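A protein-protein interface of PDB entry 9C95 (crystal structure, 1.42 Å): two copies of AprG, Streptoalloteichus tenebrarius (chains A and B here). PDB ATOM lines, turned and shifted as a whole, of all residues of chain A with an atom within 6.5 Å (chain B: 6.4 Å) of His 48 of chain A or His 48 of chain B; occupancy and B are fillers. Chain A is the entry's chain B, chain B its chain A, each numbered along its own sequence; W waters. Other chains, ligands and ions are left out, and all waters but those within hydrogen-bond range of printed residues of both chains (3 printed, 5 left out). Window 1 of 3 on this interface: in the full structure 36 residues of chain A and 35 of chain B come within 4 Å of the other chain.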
ATOM      1  N   GLY A  43      -3.178  -6.292 -27.302  1.00  0.00           N
ATOM      2  CA  GLY A  43      -4.013  -5.349 -28.046  1.00  0.00           C
ATOM      3  C   GLY A  43      -3.846  -3.910 -27.626  1.00  0.00           C
ATOM      4  O   GLY A  43      -3.827  -3.021 -28.484  1.00  0.00           O
ATOM      5  N   MET A  44      -3.766  -3.619 -26.328  1.00  0.00           N
ATOM      6  CA  MET A  44      -3.644  -2.222 -25.903  1.00  0.00           C
ATOM      7  C   MET A  44      -2.390  -1.593 -26.479  1.00  0.00           C
ATOM      8  O   MET A  44      -2.430  -0.502 -27.073  1.00  0.00           O
ATOM      9  CB  MET A  44      -3.547  -2.119 -24.388  1.00  0.00           C
ATOM     10  CG  MET A  44      -4.894  -2.155 -23.659  1.00  0.00           C
ATOM     11  SD  MET A  44      -4.693  -1.974 -21.856  1.00  0.00           S
ATOM     12  CE  MET A  44      -3.906  -3.535 -21.426  1.00  0.00           C
ATOM     13  N   TRP A  45      -1.256  -2.274 -26.325  1.00  0.00           N
ATOM     14  CA  TRP A  45       0.003  -1.729 -26.814  1.00  0.00           C
ATOM     15  C   TRP A  45       0.000  -1.630 -28.342  1.00  0.00           C
ATOM     16  O   TRP A  45       0.340  -0.573 -28.894  1.00  0.00           O
ATOM     17  CB  TRP A  45       1.158  -2.573 -26.298  1.00  0.00           C
ATOM     18  CG  TRP A  45       2.505  -1.944 -26.462  1.00  0.00           C
ATOM     19  CD1 TRP A  45       2.795  -0.659 -26.805  1.00  0.00           C
ATOM     20  CD2 TRP A  45       3.748  -2.613 -26.306  1.00  0.00           C
ATOM     21  NE1 TRP A  45       4.167  -0.486 -26.850  1.00  0.00           N
ATOM     22  CE2 TRP A  45       4.771  -1.674 -26.570  1.00  0.00           C
ATOM     23  CE3 TRP A  45       4.092  -3.914 -25.968  1.00  0.00           C
ATOM     24  CZ2 TRP A  45       6.124  -2.017 -26.499  1.00  0.00           C
ATOM     25  CZ3 TRP A  45       5.418  -4.245 -25.884  1.00  0.00           C
ATOM     26  CH2 TRP A  45       6.416  -3.291 -26.169  1.00  0.00           C
ATOM     27  N   ALA A  46      -0.426  -2.696 -29.035  1.00  0.00           N
ATOM     28  CA  ALA A  46      -0.424  -2.689 -30.513  1.00  0.00           C
ATOM     29  C   ALA A  46      -1.315  -1.584 -31.070  1.00  0.00           C
ATOM     30  O   ALA A  46      -0.916  -0.836 -31.985  1.00  0.00           O
ATOM     31  CB  ALA A  46      -0.866  -4.047 -31.058  1.00  0.00           C
ATOM     32  N   LEU A  47      -2.536  -1.475 -30.556  1.00  0.00           N
ATOM     33  CA  LEU A  47      -3.462  -0.486 -31.107  1.00  0.00           C
ATOM     34  C   LEU A  47      -3.020   0.936 -30.780  1.00  0.00           C
ATOM     35  O   LEU A  47      -3.217   1.842 -31.601  1.00  0.00           O
ATOM     36  CB  LEU A  47      -4.894  -0.754 -30.617  1.00  0.00           C
ATOM     37  CG  LEU A  47      -5.525  -2.023 -31.205  1.00  0.00           C
ATOM     38  CD1 LEU A  47      -6.834  -2.310 -30.503  1.00  0.00           C
ATOM     39  CD2 LEU A  47      -5.687  -1.888 -32.733  1.00  0.00           C
ATOM     40  N   HIS A  48      -2.437   1.166 -29.602  1.00  0.00           N
ATOM     41  CA  HIS A  48      -1.885   2.482 -29.301  1.00  0.00           C
ATOM     42  C   HIS A  48      -0.768   2.856 -30.282  1.00  0.00           C
ATOM     43  O   HIS A  48      -0.752   3.983 -30.804  1.00  0.00           O
ATOM     44  CB  HIS A  48      -1.407   2.551 -27.844  1.00  0.00           C
ATOM     45  CG  HIS A  48      -0.718   3.836 -27.496  1.00  0.00           C
ATOM     46  ND1 HIS A  48      -1.377   4.955 -27.043  1.00  0.00           N
ATOM     47  CD2 HIS A  48       0.595   4.173 -27.547  1.00  0.00           C
ATOM     48  CE1 HIS A  48      -0.510   5.932 -26.833  1.00  0.00           C
ATOM     49  NE2 HIS A  48       0.692   5.482 -27.128  1.00  0.00           N
ATOM     50  N   THR A  49       0.173   1.931 -30.558  1.00  0.00           N
ATOM     51  CA  THR A  49       1.245   2.251 -31.507  1.00  0.00           C
ATOM     52  C   THR A  49       0.698   2.568 -32.883  1.00  0.00           C
ATOM     53  O   THR A  49       1.308   3.339 -33.626  1.00  0.00           O
ATOM     54  CB  THR A  49       2.268   1.122 -31.606  1.00  0.00           C
ATOM     55  OG1 THR A  49       1.793   0.067 -32.467  1.00  0.00           O
ATOM     56  CG2 THR A  49       2.609   0.610 -30.222  1.00  0.00           C
ATOM     57  N   ALA A  50      -0.454   2.005 -33.239  1.00  0.00           N
ATOM     58  CA  ALA A  50      -1.067   2.295 -34.528  1.00  0.00           C
ATOM     59  C   ALA A  50      -1.891   3.567 -34.515  1.00  0.00           C
ATOM     60  O   ALA A  50      -2.488   3.906 -35.536  1.00  0.00           O
ATOM     61  CB  ALA A  50      -1.926   1.110 -34.935  1.00  0.00           C
ATOM     62  N   GLY A  51      -1.963   4.257 -33.379  1.00  0.00           N
ATOM     63  CA  GLY A  51      -2.722   5.485 -33.256  1.00  0.00           C
ATOM     64  C   GLY A  51      -4.191   5.279 -32.995  1.00  0.00           C
ATOM     65  O   GLY A  51      -4.944   6.259 -32.972  1.00  0.00           O
ATOM     66  N   HIS A  52      -4.627   4.038 -32.784  1.00  0.00           N
ATOM     67  CA  HIS A  52      -6.037   3.739 -32.532  1.00  0.00           C
ATOM     68  C   HIS A  52      -6.265   3.728 -31.020  1.00  0.00           C
ATOM     69  O   HIS A  52      -6.485   2.687 -30.387  1.00  0.00           O
ATOM     70  CB  HIS A  52      -6.431   2.401 -33.135  1.00  0.00           C
ATOM     71  CG  HIS A  52      -6.570   2.424 -34.614  1.00  0.00           C
ATOM     72  ND1 HIS A  52      -7.703   2.901 -35.246  1.00  0.00           N
ATOM     73  CD2 HIS A  52      -5.731   2.010 -35.588  1.00  0.00           C
ATOM     74  CE1 HIS A  52      -7.537   2.797 -36.554  1.00  0.00           C
ATOM     75  NE2 HIS A  52      -6.349   2.272 -36.789  1.00  0.00           N
ATOM     76  N   THR A  53      -6.215   4.934 -30.448  1.00  0.00           N
ATOM     77  CA  THR A  53      -6.166   5.056 -28.999  1.00  0.00           C
ATOM     78  C   THR A  53      -7.539   4.840 -28.378  1.00  0.00           C
ATOM     79  O   THR A  53      -7.615   4.399 -27.240  1.00  0.00           O
ATOM     80  CB  THR A  53      -5.624   6.435 -28.606  1.00  0.00           C
ATOM     81  OG1 THR A  53      -6.361   7.410 -29.338  1.00  0.00           O
ATOM     82  CG2 THR A  53      -4.152   6.540 -29.052  1.00  0.00           C
ATOM     83  N   ALA A  56      -7.693   1.124 -28.300  1.00  0.00           N
ATOM     84  CA  ALA A  56      -6.801   0.619 -27.267  1.00  0.00           C
ATOM     85  C   ALA A  56      -7.405   0.839 -25.892  1.00  0.00           C
ATOM     86  O   ALA A  56      -7.328  -0.038 -25.015  1.00  0.00           O
ATOM     87  CB  ALA A  56      -5.456   1.336 -27.367  1.00  0.00           C
ATOM     88  N   GLY A  97       0.903  -1.959 -22.096  1.00  0.00           N
ATOM     89  CA  GLY A  97      -0.151  -1.255 -22.805  1.00  0.00           C
ATOM     90  C   GLY A  97      -0.933  -0.300 -21.918  1.00  0.00           C
ATOM     91  O   GLY A  97      -1.230   0.830 -22.312  1.00  0.00           O
ATOM     92  N   VAL A 100       1.426   2.848 -21.107  1.00  0.00           N
ATOM     93  CA  VAL A 100       1.619   3.823 -22.180  1.00  0.00           C
ATOM     94  C   VAL A 100       0.330   4.573 -22.500  1.00  0.00           C
ATOM     95  O   VAL A 100       0.386   5.710 -22.993  1.00  0.00           O
ATOM     96  CB  VAL A 100       2.275   3.201 -23.406  1.00  0.00           C
ATOM     97  CG1 VAL A 100       3.614   2.543 -23.039  1.00  0.00           C
ATOM     98  CG2 VAL A 100       1.369   2.286 -24.090  1.00  0.00           C
ATOM     99  N   LEU A 101      -0.843   3.982 -22.224  1.00  0.00           N
ATOM    100  CA  LEU A 101      -2.110   4.714 -22.310  1.00  0.00           C
ATOM    101  C   LEU A 101      -2.317   5.706 -21.179  1.00  0.00           C
ATOM    102  O   LEU A 101      -3.344   6.427 -21.174  1.00  0.00           O
ATOM    103  CB  LEU A 101      -3.283   3.738 -22.299  1.00  0.00           C
ATOM    104  CG  LEU A 101      -3.571   3.066 -23.646  1.00  0.00           C
ATOM    105  CD1 LEU A 101      -4.549   1.885 -23.397  1.00  0.00           C
ATOM    106  CD2 LEU A 101      -4.143   4.099 -24.668  1.00  0.00           C
ATOM    107  N   ASP A 322       5.823  -2.187 -36.428  1.00  0.00           N
ATOM    108  CA  ASP A 322       6.016  -0.802 -36.028  1.00  0.00           C
ATOM    109  C   ASP A 322       7.384  -0.588 -35.378  1.00  0.00           C
ATOM    110  O   ASP A 322       8.099   0.364 -35.720  1.00  0.00           O
ATOM    111  CB  ASP A 322       4.907  -0.392 -35.062  1.00  0.00           C
ATOM    112  CG  ASP A 322       5.046   1.057 -34.671  1.00  0.00           C
ATOM    113  OD1 ASP A 322       5.901   1.327 -33.808  1.00  0.00           O
ATOM    114  OD2 ASP A 322       4.378   1.926 -35.277  1.00  0.00           O
ATOM    115  N   ARG A 326      10.400   1.738 -36.957  1.00  0.00           N
ATOM    116  CA  ARG A 326      10.892   3.005 -36.436  1.00  0.00           C
ATOM    117  C   ARG A 326      12.355   2.926 -36.048  1.00  0.00           C
ATOM    118  O   ARG A 326      13.070   3.910 -36.203  1.00  0.00           O
ATOM    119  CB  ARG A 326      10.009   3.575 -35.353  1.00  0.00           C
ATOM    120  CG  ARG A 326      10.064   2.787 -34.124  1.00  0.00           C
ATOM    121  CD  ARG A 326       8.764   3.017 -33.375  1.00  0.00           C
ATOM    122  NE  ARG A 326       8.912   2.891 -31.931  1.00  0.00           N
ATOM    123  CZ  ARG A 326       7.909   2.709 -31.050  1.00  0.00           C
ATOM    124  NH1 ARG A 326       6.678   2.507 -31.421  1.00  0.00           N
ATOM    125  NH2 ARG A 326       8.155   2.682 -29.765  1.00  0.00           N
ATOM    126  N   GLY B  43       6.025  17.279 -29.847  1.00  0.00           N
ATOM    127  CA  GLY B  43       5.902  16.493 -31.061  1.00  0.00           C
ATOM    128  C   GLY B  43       6.032  14.992 -30.879  1.00  0.00           C
ATOM    129  O   GLY B  43       5.294  14.232 -31.509  1.00  0.00           O
ATOM    130  N   MET B  44       6.981  14.530 -30.060  1.00  0.00           N
ATOM    131  CA  MET B  44       7.128  13.082 -29.888  1.00  0.00           C
ATOM    132  C   MET B  44       5.848  12.468 -29.352  1.00  0.00           C
ATOM    133  O   MET B  44       5.360  11.454 -29.874  1.00  0.00           O
ATOM    134  CB  MET B  44       8.259  12.742 -28.901  1.00  0.00           C
ATOM    135  CG  MET B  44       9.663  12.771 -29.507  1.00  0.00           C
ATOM    136  SD  MET B  44      10.956  12.329 -28.293  1.00  0.00           S
ATOM    137  CE  MET B  44      10.849  13.762 -27.214  1.00  0.00           C
ATOM    138  N   TRP B  45       5.320  13.046 -28.270  1.00  0.00           N
ATOM    139  CA  TRP B  45       4.128  12.489 -27.662  1.00  0.00           C
ATOM    140  C   TRP B  45       2.935  12.619 -28.608  1.00  0.00           C
ATOM    141  O   TRP B  45       2.198  11.649 -28.818  1.00  0.00           O
ATOM    142  CB  TRP B  45       3.890  13.174 -26.319  1.00  0.00           C
ATOM    143  CG  TRP B  45       2.843  12.545 -25.450  1.00  0.00           C
ATOM    144  CD1 TRP B  45       2.268  11.323 -25.628  1.00  0.00           C
ATOM    145  CD2 TRP B  45       2.262  13.102 -24.258  1.00  0.00           C
ATOM    146  NE1 TRP B  45       1.358  11.079 -24.608  1.00  0.00           N
ATOM    147  CE2 TRP B  45       1.333  12.160 -23.776  1.00  0.00           C
ATOM    148  CE3 TRP B  45       2.436  14.299 -23.572  1.00  0.00           C
ATOM    149  CZ2 TRP B  45       0.581  12.376 -22.619  1.00  0.00           C
ATOM    150  CZ3 TRP B  45       1.702  14.515 -22.413  1.00  0.00           C
ATOM    151  CH2 TRP B  45       0.770  13.561 -21.962  1.00  0.00           C
ATOM    152  N   ALA B  46       2.734  13.796 -29.217  1.00  0.00           N
ATOM    153  CA  ALA B  46       1.575  13.970 -30.087  1.00  0.00           C
ATOM    154  C   ALA B  46       1.626  13.007 -31.273  1.00  0.00           C
ATOM    155  O   ALA B  46       0.610  12.385 -31.632  1.00  0.00           O
ATOM    156  CB  ALA B  46       1.532  15.422 -30.580  1.00  0.00           C
ATOM    157  N   LEU B  47       2.794  12.910 -31.927  1.00  0.00           N
ATOM    158  CA  LEU B  47       2.867  12.097 -33.126  1.00  0.00           C
ATOM    159  C   LEU B  47       2.735  10.616 -32.796  1.00  0.00           C
ATOM    160  O   LEU B  47       2.115   9.870 -33.568  1.00  0.00           O
ATOM    161  CB  LEU B  47       4.154  12.396 -33.904  1.00  0.00           C
ATOM    162  CG  LEU B  47       4.116  13.769 -34.557  1.00  0.00           C
ATOM    163  CD1 LEU B  47       5.496  14.036 -35.122  1.00  0.00           C
ATOM    164  CD2 LEU B  47       3.094  13.715 -35.682  1.00  0.00           C
ATOM    165  N   HIS B  48       3.244  10.189 -31.635  1.00  0.00           N
ATOM    166  CA  HIS B  48       3.036   8.805 -31.214  1.00  0.00           C
ATOM    167  C   HIS B  48       1.547   8.518 -30.996  1.00  0.00           C
ATOM    168  O   HIS B  48       1.039   7.498 -31.477  1.00  0.00           O
ATOM    169  CB  HIS B  48       3.879   8.556 -29.963  1.00  0.00           C
ATOM    170  CG  HIS B  48       3.731   7.180 -29.376  1.00  0.00           C
ATOM    171  ND1 HIS B  48       4.247   6.042 -29.943  1.00  0.00           N
ATOM    172  CD2 HIS B  48       3.058   6.772 -28.274  1.00  0.00           C
ATOM    173  CE1 HIS B  48       3.940   4.991 -29.197  1.00  0.00           C
ATOM    174  NE2 HIS B  48       3.217   5.406 -28.182  1.00  0.00           N
ATOM    175  N   THR B  49       0.812   9.428 -30.319  1.00  0.00           N
ATOM    176  CA  THR B  49      -0.631   9.191 -30.118  1.00  0.00           C
ATOM    177  C   THR B  49      -1.374   9.056 -31.438  1.00  0.00           C
ATOM    178  O   THR B  49      -2.388   8.356 -31.526  1.00  0.00           O
ATOM    179  CB  THR B  49      -1.311  10.280 -29.257  1.00  0.00           C
ATOM    180  OG1 THR B  49      -1.560  11.465 -30.048  1.00  0.00           O
ATOM    181  CG2 THR B  49      -0.458  10.537 -28.027  1.00  0.00           C
ATOM    182  N   ALA B  50      -0.917   9.755 -32.477  1.00  0.00           N
ATOM    183  CA  ALA B  50      -1.534   9.643 -33.778  1.00  0.00           C
ATOM    184  C   ALA B  50      -1.056   8.438 -34.581  1.00  0.00           C
ATOM    185  O   ALA B  50      -1.483   8.249 -35.722  1.00  0.00           O
ATOM    186  CB  ALA B  50      -1.253  10.923 -34.565  1.00  0.00           C
ATOM    187  N   GLY B  51      -0.201   7.600 -34.017  1.00  0.00           N
ATOM    188  CA  GLY B  51       0.273   6.435 -34.752  1.00  0.00           C
ATOM    189  C   GLY B  51       1.449   6.700 -35.656  1.00  0.00           C
ATOM    190  O   GLY B  51       1.903   5.775 -36.336  1.00  0.00           O
ATOM    191  N   HIS B  52       1.953   7.934 -35.683  1.00  0.00           N
ATOM    192  CA  HIS B  52       3.044   8.275 -36.599  1.00  0.00           C
ATOM    193  C   HIS B  52       4.365   8.063 -35.875  1.00  0.00           C
ATOM    194  O   HIS B  52       5.077   9.006 -35.510  1.00  0.00           O
ATOM    195  CB  HIS B  52       2.911   9.716 -37.070  1.00  0.00           C
ATOM    196  CG  HIS B  52       1.884   9.899 -38.139  1.00  0.00           C
ATOM    197  ND1 HIS B  52       2.153   9.653 -39.472  1.00  0.00           N
ATOM    198  CD2 HIS B  52       0.608  10.342 -38.080  1.00  0.00           C
ATOM    199  CE1 HIS B  52       1.074   9.935 -40.185  1.00  0.00           C
ATOM    200  NE2 HIS B  52       0.133  10.374 -39.372  1.00  0.00           N
ATOM    201  N   THR B  53       4.672   6.778 -35.641  1.00  0.00           N
ATOM    202  CA  THR B  53       5.797   6.462 -34.758  1.00  0.00           C
ATOM    203  C   THR B  53       7.163   6.685 -35.413  1.00  0.00           C
ATOM    204  O   THR B  53       8.144   6.959 -34.703  1.00  0.00           O
ATOM    205  CB  THR B  53       5.679   5.013 -34.269  1.00  0.00           C
ATOM    206  OG1 THR B  53       5.468   4.186 -35.407  1.00  0.00           O
ATOM    207  CG2 THR B  53       4.464   4.867 -33.335  1.00  0.00           C
ATOM    208  N   ALA B  56       7.549  10.364 -34.978  1.00  0.00           N
ATOM    209  CA  ALA B  56       7.842  10.646 -33.583  1.00  0.00           C
ATOM    210  C   ALA B  56       9.260  10.257 -33.236  1.00  0.00           C
ATOM    211  O   ALA B  56       9.959  10.986 -32.516  1.00  0.00           O
ATOM    212  CB  ALA B  56       6.863   9.876 -32.696  1.00  0.00           C
ATOM    213  N   GLY B  97       7.244  12.078 -24.040  1.00  0.00           N
ATOM    214  CA  GLY B  97       7.270  11.551 -25.392  1.00  0.00           C
ATOM    215  C   GLY B  97       8.383  10.541 -25.591  1.00  0.00           C
ATOM    216  O   GLY B  97       8.176   9.496 -26.198  1.00  0.00           O
ATOM    217  N   VAL B 100       7.319   7.136 -23.624  1.00  0.00           N
ATOM    218  CA  VAL B 100       6.281   6.317 -24.257  1.00  0.00           C
ATOM    219  C   VAL B 100       6.778   5.679 -25.546  1.00  0.00           C
ATOM    220  O   VAL B 100       6.266   4.635 -25.951  1.00  0.00           O
ATOM    221  CB  VAL B 100       4.962   7.093 -24.466  1.00  0.00           C
ATOM    222  CG1 VAL B 100       4.414   7.605 -23.126  1.00  0.00           C
ATOM    223  CG2 VAL B 100       5.150   8.199 -25.483  1.00  0.00           C
ATOM    224  N   LEU B 101       7.761   6.298 -26.223  1.00  0.00           N
ATOM    225  CA  LEU B 101       8.401   5.709 -27.388  1.00  0.00           C
ATOM    226  C   LEU B 101       9.366   4.604 -27.020  1.00  0.00           C
ATOM    227  O   LEU B 101       9.898   3.953 -27.914  1.00  0.00           O
ATOM    228  CB  LEU B 101       9.223   6.758 -28.156  1.00  0.00           C
ATOM    229  CG  LEU B 101       8.454   7.566 -29.211  1.00  0.00           C
ATOM    230  CD1 LEU B 101       9.302   8.700 -29.744  1.00  0.00           C
ATOM    231  CD2 LEU B 101       7.944   6.682 -30.386  1.00  0.00           C
ATOM    232  N   ASP B 322      -6.885  13.804 -29.026  1.00  0.00           N
ATOM    233  CA  ASP B 322      -6.765  12.371 -28.799  1.00  0.00           C
ATOM    234  C   ASP B 322      -7.136  12.005 -27.366  1.00  0.00           C
ATOM    235  O   ASP B 322      -7.933  11.088 -27.141  1.00  0.00           O
ATOM    236  CB  ASP B 322      -5.358  11.903 -29.109  1.00  0.00           C
ATOM    237  CG  ASP B 322      -5.218  10.428 -28.883  1.00  0.00           C
ATOM    238  OD1 ASP B 322      -4.993  10.037 -27.727  1.00  0.00           O
ATOM    239  OD2 ASP B 322      -5.428   9.645 -29.830  1.00  0.00           O
ATOM    240  N   ARG B 326     -10.418   9.774 -26.275  1.00  0.00           N
ATOM    241  CA  ARG B 326     -10.373   8.440 -25.687  1.00  0.00           C
ATOM    242  C   ARG B 326     -10.978   8.387 -24.292  1.00  0.00           C
ATOM    243  O   ARG B 326     -11.625   7.387 -23.963  1.00  0.00           O
ATOM    244  CB  ARG B 326      -9.011   7.802 -25.803  1.00  0.00           C
ATOM    245  CG  ARG B 326      -8.050   8.365 -24.871  1.00  0.00           C
ATOM    246  CD  ARG B 326      -6.692   8.019 -25.454  1.00  0.00           C
ATOM    247  NE  ARG B 326      -5.677   7.999 -24.445  1.00  0.00           N
ATOM    248  CZ  ARG B 326      -4.367   8.112 -24.681  1.00  0.00           C
ATOM    249  NH1 ARG B 326      -3.520   8.007 -23.677  1.00  0.00           N
ATOM    250  NH2 ARG B 326      -3.890   8.388 -25.881  1.00  0.00           N
HETATM  251  O   HOH W   1      -8.716   9.315 -29.248  1.00  0.00           O
HETATM  252  O   HOH W   2      -0.688   8.139 -22.747  1.00  0.00           O
HETATM  253  O   HOH W   3       7.010   2.480 -37.319  1.00  0.00           O
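NE2 of His 48 of chain A lies within hydrogen-bond range of NE2 of His 48 of chain B (2.7 Å).
OD2 of Asp 322 of chain A sits at hydrogen-bond distance from OG1 of Thr 53 of chain B (2.5 Å).
The guanidinium group (NH2) of Arg 326 of chain A is in hydrogen-bond range of the backbone carbonyl oxygen (O) of Leu 101 of chain B.
OD2 of Asp 322 of chain B lies within hydrogen-bond range of OG1 of Thr 53 of chain A (2.5 Å).
The backbone carbonyl oxygen of Leu 101 of chain A lies within hydrogen-bond range of the guanidinium group of Arg 326 of chain B (3.0 Å).
The backbone carbonyl oxygen of Ala 46 of chain B is in hydrogen-bond range of the side-chain hydroxyl of Thr 49 of chain B (2.8 Å).
The guanidinium group (NH2) of Arg 326 of chain B lies within salt-bridge range of the side-chain carboxylate (OD1) of Asp 322 of chain B (2.7 Å).
O of Ala 46 of chain A sits at hydrogen-bond distance from OG1 of Thr 49 of chain A (2.9 Å).
The side-chain carboxylate (OD1) of Asp 322 of chain A is in salt-bridge range of the guanidinium group (NH1) of Arg 326 of chain A, at 2.8 Å.
Thr 49 of chain A touches Gly 51 of chain B.
Thr 53 of chain B touches Thr 49 of chain A (CG2 to O, 3.5 Å).
Gly 51 of chain B touches Ala 50 of chain A.
Gly 51 of chain A touches Thr 49 of chain B (CA to O, 3.4 Å).
Gly 51 of chain A touches Ala 50 of chain B (CA to C, 3.6 Å).
CA of Gly 51 of chain A touches N of Gly 51 of chain B, at 3.4 Å.
Thr 49 of chain B touches Thr 53 of chain A.
CG2 of Thr 53 of chain A touches NH2 of Arg 326 of chain B (3.7 Å).
Arg 326 of chain A touches Thr 53 of chain B (NH1 to CG2, 3.8 Å).
Printed residues of chain B within 4 Å of His 48 of chain A: His 48 (2.7 Å).
Printed residues of chain B within 4 Å of Gly 51 of chain A: Thr 49, Ala 50 and Gly 51.
Gly 97 of chain A touches none of the printed residues of chain B.
Val 100 of chain A touches none of the printed residues of chain B.
Of the printed residues of chain B, Leu 101 of chain A touches Arg 326 (3.0 Å).
Of chain A, only His 48 comes within 4 Å of His 48 of chain B.
Of the printed residues of chain A, Arg 326 of chain B touches Thr 53 and Leu 101.
The nearest residue of chain B that does not touch His 48 of chain A is Arg 326 of chain B (4.3 Å).
The nearest residue of chain A that does not touch His 48 of chain B is Arg 326 of chain A (4.3 Å).
Printed residues of chain A that touch a printed residue of chain B: His 48, Thr 49, Ala 50, Gly 51, Thr 53, Leu 101, Asp 322 and Arg 326.
Printed residues of chain B that touch a printed residue of chain A: His 48, Thr 49, Ala 50, Gly 51, Thr 53, Leu 101, Asp 322 and Arg 326.
Hydrophobic or aromatic side chains of chain B that line the printed part of chain A: His 48.
Along chain B the printed residues that touch a printed residue of chain A span positions 48 to 326.
Among the printed residues, 14 pairs touch across the chains.
Thr 49 of chain A touches Thr 53 of chain B, and with the chains exchanged Thr 53 of chain A touches Thr 49 of chain B.
Ala 50 of chain A touches Gly 51 of chain B, and with the chains exchanged Gly 51 of chain A touches Ala 50 of chain B.
Thr 53 of chain A touches Asp 322 of chain B, and with the chains exchanged Asp 322 of chain A touches Thr 53 of chain B.
Leu 101 of chain A touches Arg 326 of chain B, and with the chains exchanged Arg 326 of chain A touches Leu 101 of chain B.
Water W2 bridges O of Val 100 of chain A and NH1 of Arg 326 of chain B.
Water W1 lies within hydrogen-bond range of O of Asp 322 of chain B (2.9 Å), OG1 of Thr 53 of chain A (3.0 Å) and N of Arg 326 of chain B (3.5 Å).
Water W3 lies within hydrogen-bond range of the backbone carbonyl oxygen (O) of Asp 322 of chain A (2.9 Å), the side-chain hydroxyl (OG1) of Thr 53 of chain B (3.0 Å) and the backbone NH (N) of Arg 326 of chain A (3.5 Å).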
